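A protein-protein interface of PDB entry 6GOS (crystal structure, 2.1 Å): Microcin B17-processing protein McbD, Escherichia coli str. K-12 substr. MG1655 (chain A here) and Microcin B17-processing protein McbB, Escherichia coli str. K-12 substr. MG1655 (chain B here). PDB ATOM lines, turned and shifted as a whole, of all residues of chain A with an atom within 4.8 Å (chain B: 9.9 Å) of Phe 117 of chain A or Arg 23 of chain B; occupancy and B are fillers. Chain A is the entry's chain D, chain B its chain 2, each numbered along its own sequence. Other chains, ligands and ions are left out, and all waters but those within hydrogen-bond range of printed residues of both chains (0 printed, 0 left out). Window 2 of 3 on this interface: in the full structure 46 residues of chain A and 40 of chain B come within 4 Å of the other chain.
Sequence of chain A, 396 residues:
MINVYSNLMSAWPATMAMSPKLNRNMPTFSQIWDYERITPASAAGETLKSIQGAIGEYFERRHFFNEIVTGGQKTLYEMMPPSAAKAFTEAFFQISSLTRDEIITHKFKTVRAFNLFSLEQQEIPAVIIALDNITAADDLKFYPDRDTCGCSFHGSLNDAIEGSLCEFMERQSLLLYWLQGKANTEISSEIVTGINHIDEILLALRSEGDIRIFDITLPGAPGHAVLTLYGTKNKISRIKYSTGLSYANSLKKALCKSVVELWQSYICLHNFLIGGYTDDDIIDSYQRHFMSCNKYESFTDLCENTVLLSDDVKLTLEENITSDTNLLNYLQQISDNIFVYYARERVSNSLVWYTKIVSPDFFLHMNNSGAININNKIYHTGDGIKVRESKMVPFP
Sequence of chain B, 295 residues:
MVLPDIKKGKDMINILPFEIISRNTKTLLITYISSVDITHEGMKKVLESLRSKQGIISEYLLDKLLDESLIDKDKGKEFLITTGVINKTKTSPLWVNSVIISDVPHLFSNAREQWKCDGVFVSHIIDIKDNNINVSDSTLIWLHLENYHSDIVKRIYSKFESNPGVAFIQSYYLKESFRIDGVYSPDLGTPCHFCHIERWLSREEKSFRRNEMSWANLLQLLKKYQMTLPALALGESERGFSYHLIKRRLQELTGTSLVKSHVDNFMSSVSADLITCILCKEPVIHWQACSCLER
NH1 of Arg 23 of chain B sits at hydrogen-bond distance from O of Leu 116 of chain A, at 2.9 Å.
N of Leu 28 of chain B lies within hydrogen-bond range of O of Ile 21 of chain B, 2.9 Å away.
The backbone NH of Leu 116 of chain A sits at hydrogen-bond distance from the backbone carbonyl oxygen of Ile 338 of chain A (2.8 Å).
OD1 of Asn 115 of chain A lies within hydrogen-bond range of N of Ser 118 of chain A (3.0 Å).
OD1 of Asn 115 of chain A sits at hydrogen-bond distance from N of Phe 117 of chain A (2.9 Å).
Arg 23 of chain B touches Phe 117 of chain A.
Ser 118 of chain A touches Lys 26 of chain B (O to CB, 3.9 Å).
CD1 of Leu 119 of chain A touches O of Ile 21 of chain B, 3.2 Å away.
Leu 119 of chain A touches Arg 23 of chain B (CD1 to N, 3.9 Å).
CD1 of Leu 119 of chain A touches O of Lys 26 of chain B, at 3.9 Å.
Leu 28 of chain B touches Leu 119 of chain A.
CD1 of Leu 328 of chain A touches NH1 of Arg 23 of chain B (3.3 Å).
No residue of chain B comes within 4 Å of Asn 115 of chain A.
Leu 116 of chain A touches one residue of chain B.
Of chain B, only Arg 23 (3.3 Å) comes within 4 Å of Phe 117 of chain A.
Printed residues of chain B within 4 Å of Leu 119 of chain A: Ile 21, Arg 23, Lys 26 and Leu 28.
No residue of chain B comes within 4 Å of Gln 332 of chain A.
No residue of chain B comes within 4 Å of Ile 338 of chain A.
Of the printed residues of chain A, Ile 21 of chain B touches Leu 119.
Arg 23 of chain B touches four residues of chain A.
Thr 25 of chain B touches none of the printed residues of chain A.
Of the printed residues of chain A, Lys 26 of chain B touches Ser 118 (3.9 Å) and Leu 119 (3.9 Å).
Printed residues of chain A within 4 Å of Leu 28 of chain B: Leu 119.
The nearest residue of chain B that does not touch Phe 117 of chain A is Asn 24 of chain B (5.8 Å).
The nearest printed residue of chain A that does not touch Ile 21 of chain B is Leu 116 of chain A (5.9 Å).
Printed residues of chain A that touch a printed residue of chain B: Leu 116, Phe 117, Ser 118, Leu 119 and Leu 328.
Among the printed residues, 8 pairs touch across the chains.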
ATOM      1  N   ASN A 115      -8.051   5.061  -6.372  1.00  0.00           N
ATOM      2  CA  ASN A 115      -8.439   4.977  -7.788  1.00  0.00           C
ATOM      3  C   ASN A 115      -7.169   4.999  -8.660  1.00  0.00           C
ATOM      4  O   ASN A 115      -6.310   5.879  -8.494  1.00  0.00           O
ATOM      5  CB  ASN A 115      -9.393   6.136  -8.145  1.00  0.00           C
ATOM      6  CG  ASN A 115      -9.848   6.111  -9.599  1.00  0.00           C
ATOM      7  OD1 ASN A 115      -9.114   6.530 -10.507  1.00  0.00           O
ATOM      8  ND2 ASN A 115     -11.066   5.626  -9.827  1.00  0.00           N
ATOM      9  N   LEU A 116      -7.064   4.045  -9.590  1.00  0.00           N
ATOM     10  CA  LEU A 116      -5.862   3.904 -10.444  1.00  0.00           C
ATOM     11  C   LEU A 116      -5.480   5.183 -11.199  1.00  0.00           C
ATOM     12  O   LEU A 116      -4.286   5.427 -11.441  1.00  0.00           O
ATOM     13  CB  LEU A 116      -6.042   2.764 -11.457  1.00  0.00           C
ATOM     14  CG  LEU A 116      -4.870   2.420 -12.390  1.00  0.00           C
ATOM     15  CD1 LEU A 116      -3.637   2.078 -11.577  1.00  0.00           C
ATOM     16  CD2 LEU A 116      -5.218   1.265 -13.333  1.00  0.00           C
ATOM     17  N   PHE A 117      -6.482   5.989 -11.559  1.00  0.00           N
ATOM     18  CA  PHE A 117      -6.273   7.141 -12.419  1.00  0.00           C
ATOM     19  C   PHE A 117      -6.205   8.478 -11.690  1.00  0.00           C
ATOM     20  O   PHE A 117      -5.361   9.299 -12.032  1.00  0.00           O
ATOM     21  CB  PHE A 117      -7.367   7.171 -13.481  1.00  0.00           C
ATOM     22  CG  PHE A 117      -7.593   5.837 -14.131  1.00  0.00           C
ATOM     23  CD1 PHE A 117      -6.608   5.276 -14.937  1.00  0.00           C
ATOM     24  CD2 PHE A 117      -8.770   5.134 -13.912  1.00  0.00           C
ATOM     25  CE1 PHE A 117      -6.798   4.040 -15.529  1.00  0.00           C
ATOM     26  CE2 PHE A 117      -8.976   3.907 -14.511  1.00  0.00           C
ATOM     27  CZ  PHE A 117      -7.994   3.358 -15.322  1.00  0.00           C
ATOM     28  N   SER A 118      -7.090   8.712 -10.720  1.00  0.00           N
ATOM     29  CA  SER A 118      -7.166   9.998  -9.995  1.00  0.00           C
ATOM     30  C   SER A 118      -6.380  10.005  -8.680  1.00  0.00           C
ATOM     31  O   SER A 118      -6.268  11.049  -8.029  1.00  0.00           O
ATOM     32  CB  SER A 118      -8.627  10.343  -9.686  1.00  0.00           C
ATOM     33  OG  SER A 118      -9.132   9.599  -8.592  1.00  0.00           O
ATOM     34  N   LEU A 119      -5.883   8.829  -8.288  1.00  0.00           N
ATOM     35  CA  LEU A 119      -5.290   8.581  -6.982  1.00  0.00           C
ATOM     36  C   LEU A 119      -6.200   8.897  -5.785  1.00  0.00           C
ATOM     37  O   LEU A 119      -5.718   8.901  -4.652  1.00  0.00           O
ATOM     38  CB  LEU A 119      -3.928   9.276  -6.859  1.00  0.00           C
ATOM     39  CG  LEU A 119      -2.925   8.918  -7.962  1.00  0.00           C
ATOM     40  CD1 LEU A 119      -1.623   9.667  -7.722  1.00  0.00           C
ATOM     41  CD2 LEU A 119      -2.667   7.418  -8.073  1.00  0.00           C
ATOM     42  N   LEU A 328      -2.767   3.011 -19.155  1.00  0.00           N
ATOM     43  CA  LEU A 328      -3.702   3.705 -18.252  1.00  0.00           C
ATOM     44  C   LEU A 328      -4.813   4.456 -19.007  1.00  0.00           C
ATOM     45  O   LEU A 328      -5.980   4.413 -18.598  1.00  0.00           O
ATOM     46  CB  LEU A 328      -2.960   4.658 -17.294  1.00  0.00           C
ATOM     47  CG  LEU A 328      -2.018   4.088 -16.213  1.00  0.00           C
ATOM     48  CD1 LEU A 328      -1.702   5.146 -15.162  1.00  0.00           C
ATOM     49  CD2 LEU A 328      -2.598   2.854 -15.533  1.00  0.00           C
ATOM     50  N   LEU A 331      -7.205   1.764 -20.362  1.00  0.00           N
ATOM     51  CA  LEU A 331      -8.076   1.247 -19.320  1.00  0.00           C
ATOM     52  C   LEU A 331      -9.121   2.257 -18.854  1.00  0.00           C
ATOM     53  O   LEU A 331     -10.279   1.887 -18.663  1.00  0.00           O
ATOM     54  CB  LEU A 331      -7.253   0.733 -18.120  1.00  0.00           C
ATOM     55  CG  LEU A 331      -6.458  -0.562 -18.377  1.00  0.00           C
ATOM     56  CD1 LEU A 331      -5.476  -0.864 -17.247  1.00  0.00           C
ATOM     57  CD2 LEU A 331      -7.422  -1.709 -18.634  1.00  0.00           C
ATOM     58  N   GLN A 332      -8.723   3.519 -18.673  1.00  0.00           N
ATOM     59  CA  GLN A 332      -9.669   4.555 -18.217  1.00  0.00           C
ATOM     60  C   GLN A 332     -10.820   4.791 -19.203  1.00  0.00           C
ATOM     61  O   GLN A 332     -11.936   5.045 -18.781  1.00  0.00           O
ATOM     62  CB  GLN A 332      -8.968   5.882 -17.911  1.00  0.00           C
ATOM     63  CG  GLN A 332      -9.856   6.859 -17.141  1.00  0.00           C
ATOM     64  CD  GLN A 332      -9.123   8.088 -16.606  1.00  0.00           C
ATOM     65  OE1 GLN A 332      -7.975   8.367 -16.971  1.00  0.00           O
ATOM     66  NE2 GLN A 332      -9.795   8.832 -15.730  1.00  0.00           N
ATOM     67  N   SER A 335     -13.171   2.080 -18.325  1.00  0.00           N
ATOM     68  CA  SER A 335     -13.774   2.344 -17.019  1.00  0.00           C
ATOM     69  C   SER A 335     -12.904   3.215 -16.125  1.00  0.00           C
ATOM     70  O   SER A 335     -11.698   2.990 -16.040  1.00  0.00           O
ATOM     71  CB  SER A 335     -14.029   1.037 -16.278  1.00  0.00           C
ATOM     72  OG  SER A 335     -14.662   1.302 -15.037  1.00  0.00           O
ATOM     73  N   ASP A 336     -13.548   4.175 -15.451  1.00  0.00           N
ATOM     74  CA  ASP A 336     -12.963   4.928 -14.324  1.00  0.00           C
ATOM     75  C   ASP A 336     -12.837   4.109 -13.036  1.00  0.00           C
ATOM     76  O   ASP A 336     -12.075   4.480 -12.135  1.00  0.00           O
ATOM     77  CB  ASP A 336     -13.810   6.177 -13.998  1.00  0.00           C
ATOM     78  CG  ASP A 336     -13.375   7.404 -14.775  1.00  0.00           C
ATOM     79  OD1 ASP A 336     -12.186   7.774 -14.658  1.00  0.00           O
ATOM     80  OD2 ASP A 336     -14.222   8.010 -15.476  1.00  0.00           O
ATOM     81  N   ILE A 338     -11.396   1.516 -11.577  1.00  0.00           N
ATOM     82  CA  ILE A 338     -10.277   0.607 -11.406  1.00  0.00           C
ATOM     83  C   ILE A 338      -9.534   1.098 -10.161  1.00  0.00           C
ATOM     84  O   ILE A 338      -9.130   2.273 -10.072  1.00  0.00           O
ATOM     85  CB  ILE A 338      -9.349   0.528 -12.650  1.00  0.00           C
ATOM     86  CG1 ILE A 338     -10.162   0.268 -13.917  1.00  0.00           C
ATOM     87  CG2 ILE A 338      -8.326  -0.601 -12.480  1.00  0.00           C
ATOM     88  CD1 ILE A 338      -9.355  -0.049 -15.162  1.00  0.00           C
ATOM     89  N   ILE B  20       5.951   8.142  -3.350  1.00  0.00           N
ATOM     90  CA  ILE B  20       5.009   9.086  -3.938  1.00  0.00           C
ATOM     91  C   ILE B  20       4.631   8.572  -5.319  1.00  0.00           C
ATOM     92  O   ILE B  20       5.487   8.136  -6.097  1.00  0.00           O
ATOM     93  CB  ILE B  20       5.504  10.560  -4.017  1.00  0.00           C
ATOM     94  CG1 ILE B  20       6.997  10.648  -4.299  1.00  0.00           C
ATOM     95  CG2 ILE B  20       5.189  11.306  -2.724  1.00  0.00           C
ATOM     96  CD1 ILE B  20       7.443  12.037  -4.694  1.00  0.00           C
ATOM     97  N   ILE B  21       3.336   8.603  -5.604  1.00  0.00           N
ATOM     98  CA  ILE B  21       2.815   8.218  -6.916  1.00  0.00           C
ATOM     99  C   ILE B  21       2.144   9.474  -7.476  1.00  0.00           C
ATOM    100  O   ILE B  21       1.373  10.132  -6.774  1.00  0.00           O
ATOM    101  CB  ILE B  21       1.902   6.945  -6.860  1.00  0.00           C
ATOM    102  CG1 ILE B  21       1.248   6.679  -8.230  1.00  0.00           C
ATOM    103  CG2 ILE B  21       0.846   7.032  -5.752  1.00  0.00           C
ATOM    104  CD1 ILE B  21       0.738   5.259  -8.428  1.00  0.00           C
ATOM    105  N   SER B  22       2.499   9.837  -8.708  1.00  0.00           N
ATOM    106  CA  SER B  22       1.997  11.061  -9.333  1.00  0.00           C
ATOM    107  C   SER B  22       1.245  10.721 -10.602  1.00  0.00           C
ATOM    108  O   SER B  22       1.679   9.882 -11.379  1.00  0.00           O
ATOM    109  CB  SER B  22       3.137  12.034  -9.638  1.00  0.00           C
ATOM    110  OG  SER B  22       3.613  12.631  -8.445  1.00  0.00           O
ATOM    111  N   ARG B  23       0.110  11.377 -10.792  1.00  0.00           N
ATOM    112  CA  ARG B  23      -0.739  11.157 -11.955  1.00  0.00           C
ATOM    113  C   ARG B  23      -1.382  12.491 -12.314  1.00  0.00           C
ATOM    114  O   ARG B  23      -2.063  13.112 -11.473  1.00  0.00           O
ATOM    115  CB  ARG B  23      -1.782  10.075 -11.632  1.00  0.00           C
ATOM    116  CG  ARG B  23      -2.134   9.171 -12.803  1.00  0.00           C
ATOM    117  CD  ARG B  23      -2.149   7.712 -12.399  1.00  0.00           C
ATOM    118  NE  ARG B  23      -0.788   7.193 -12.264  1.00  0.00           N
ATOM    119  CZ  ARG B  23      -0.466   5.924 -12.015  1.00  0.00           C
ATOM    120  NH1 ARG B  23      -1.410   4.998 -11.850  1.00  0.00           N
ATOM    121  NH2 ARG B  23       0.819   5.574 -11.926  1.00  0.00           N
ATOM    122  N   ASN B  24      -1.129  12.948 -13.542  1.00  0.00           N
ATOM    123  CA  ASN B  24      -1.474  14.307 -13.953  1.00  0.00           C
ATOM    124  C   ASN B  24      -0.845  15.267 -12.913  1.00  0.00           C
ATOM    125  O   ASN B  24       0.349  15.124 -12.599  1.00  0.00           O
ATOM    126  CB  ASN B  24      -3.002  14.460 -14.090  1.00  0.00           C
ATOM    127  N   THR B  25      -1.636  16.184 -12.347  1.00  0.00           N
ATOM    128  CA  THR B  25      -1.176  17.063 -11.266  1.00  0.00           C
ATOM    129  C   THR B  25      -1.394  16.485  -9.852  1.00  0.00           C
ATOM    130  O   THR B  25      -1.068  17.150  -8.854  1.00  0.00           O
ATOM    131  CB  THR B  25      -1.884  18.430 -11.359  1.00  0.00           C
ATOM    132  OG1 THR B  25      -3.284  18.270 -11.098  1.00  0.00           O
ATOM    133  CG2 THR B  25      -1.680  19.045 -12.756  1.00  0.00           C
ATOM    134  N   LYS B  26      -1.942  15.269  -9.766  1.00  0.00           N
ATOM    135  CA  LYS B  26      -2.255  14.656  -8.488  1.00  0.00           C
ATOM    136  C   LYS B  26      -1.043  13.842  -7.981  1.00  0.00           C
ATOM    137  O   LYS B  26      -0.351  13.178  -8.764  1.00  0.00           O
ATOM    138  CB  LYS B  26      -3.512  13.784  -8.615  1.00  0.00           C
ATOM    139  N   THR B  27      -0.801  13.911  -6.671  1.00  0.00           N
ATOM    140  CA  THR B  27       0.299  13.191  -6.008  1.00  0.00           C
ATOM    141  C   THR B  27      -0.205  12.572  -4.693  1.00  0.00           C
ATOM    142  O   THR B  27      -0.826  13.254  -3.880  1.00  0.00           O
ATOM    143  CB  THR B  27       1.515  14.120  -5.753  1.00  0.00           C
ATOM    144  OG1 THR B  27       2.042  14.579  -7.007  1.00  0.00           O
ATOM    145  CG2 THR B  27       2.620  13.400  -5.010  1.00  0.00           C
ATOM    146  N   LEU B  28       0.059  11.277  -4.508  1.00  0.00           N
ATOM    147  CA  LEU B  28      -0.287  10.568  -3.291  1.00  0.00           C
ATOM    148  C   LEU B  28       1.001  10.099  -2.595  1.00  0.00           C
ATOM    149  O   LEU B  28       1.860   9.475  -3.227  1.00  0.00           O
ATOM    150  CB  LEU B  28      -1.215   9.389  -3.613  1.00  0.00           C
ATOM    151  CG  LEU B  28      -1.541   8.362  -2.519  1.00  0.00           C
ATOM    152  CD1 LEU B  28      -2.286   9.005  -1.359  1.00  0.00           C
ATOM    153  CD2 LEU B  28      -2.364   7.230  -3.111  1.00  0.00           C
ATOM    154  N   LEU B  29       1.100  10.416  -1.299  1.00  0.00           N
ATOM    155  CA  LEU B  29       2.218  10.069  -0.423  1.00  0.00           C
ATOM    156  C   LEU B  29       1.801   8.888   0.423  1.00  0.00           C
ATOM    157  O   LEU B  29       0.762   8.940   1.098  1.00  0.00           O
ATOM    158  CB  LEU B  29       2.565  11.245   0.511  1.00  0.00           C
ATOM    159  CG  LEU B  29       3.489  10.967   1.720  1.00  0.00           C
ATOM    160  CD1 LEU B  29       4.877  10.532   1.254  1.00  0.00           C
ATOM    161  CD2 LEU B  29       3.596  12.162   2.665  1.00  0.00           C
ATOM    162  N   ILE B  38      -1.174  15.093  -1.532  1.00  0.00           N
ATOM    163  CA  ILE B  38      -0.215  16.182  -1.501  1.00  0.00           C
ATOM    164  C   ILE B  38      -0.671  17.123  -2.596  1.00  0.00           C
ATOM    165  O   ILE B  38      -0.626  16.768  -3.767  1.00  0.00           O
ATOM    166  CB  ILE B  38       1.232  15.698  -1.792  1.00  0.00           C
ATOM    167  CG1 ILE B  38       1.645  14.552  -0.850  1.00  0.00           C
ATOM    168  CG2 ILE B  38       2.217  16.860  -1.702  1.00  0.00           C
ATOM    169  CD1 ILE B  38       1.703  14.915   0.623  1.00  0.00           C
ATOM    170  N   GLU B  48       9.840  14.889  -3.219  1.00  0.00           N
ATOM    171  CA  GLU B  48      10.515  14.330  -4.403  1.00  0.00           C
ATOM    172  C   GLU B  48      12.007  14.241  -4.168  1.00  0.00           C
ATOM    173  O   GLU B  48      12.642  13.247  -4.512  1.00  0.00           O
ATOM    174  CB  GLU B  48      10.261  15.195  -5.646  1.00  0.00           C
ATOM    175  CG  GLU B  48       9.729  14.426  -6.847  1.00  0.00           C
ATOM    176  CD  GLU B  48       8.896  15.291  -7.782  1.00  0.00           C
ATOM    177  OE1 GLU B  48       9.171  16.507  -7.910  1.00  0.00           O
ATOM    178  OE2 GLU B  48       7.952  14.749  -8.391  1.00  0.00           O
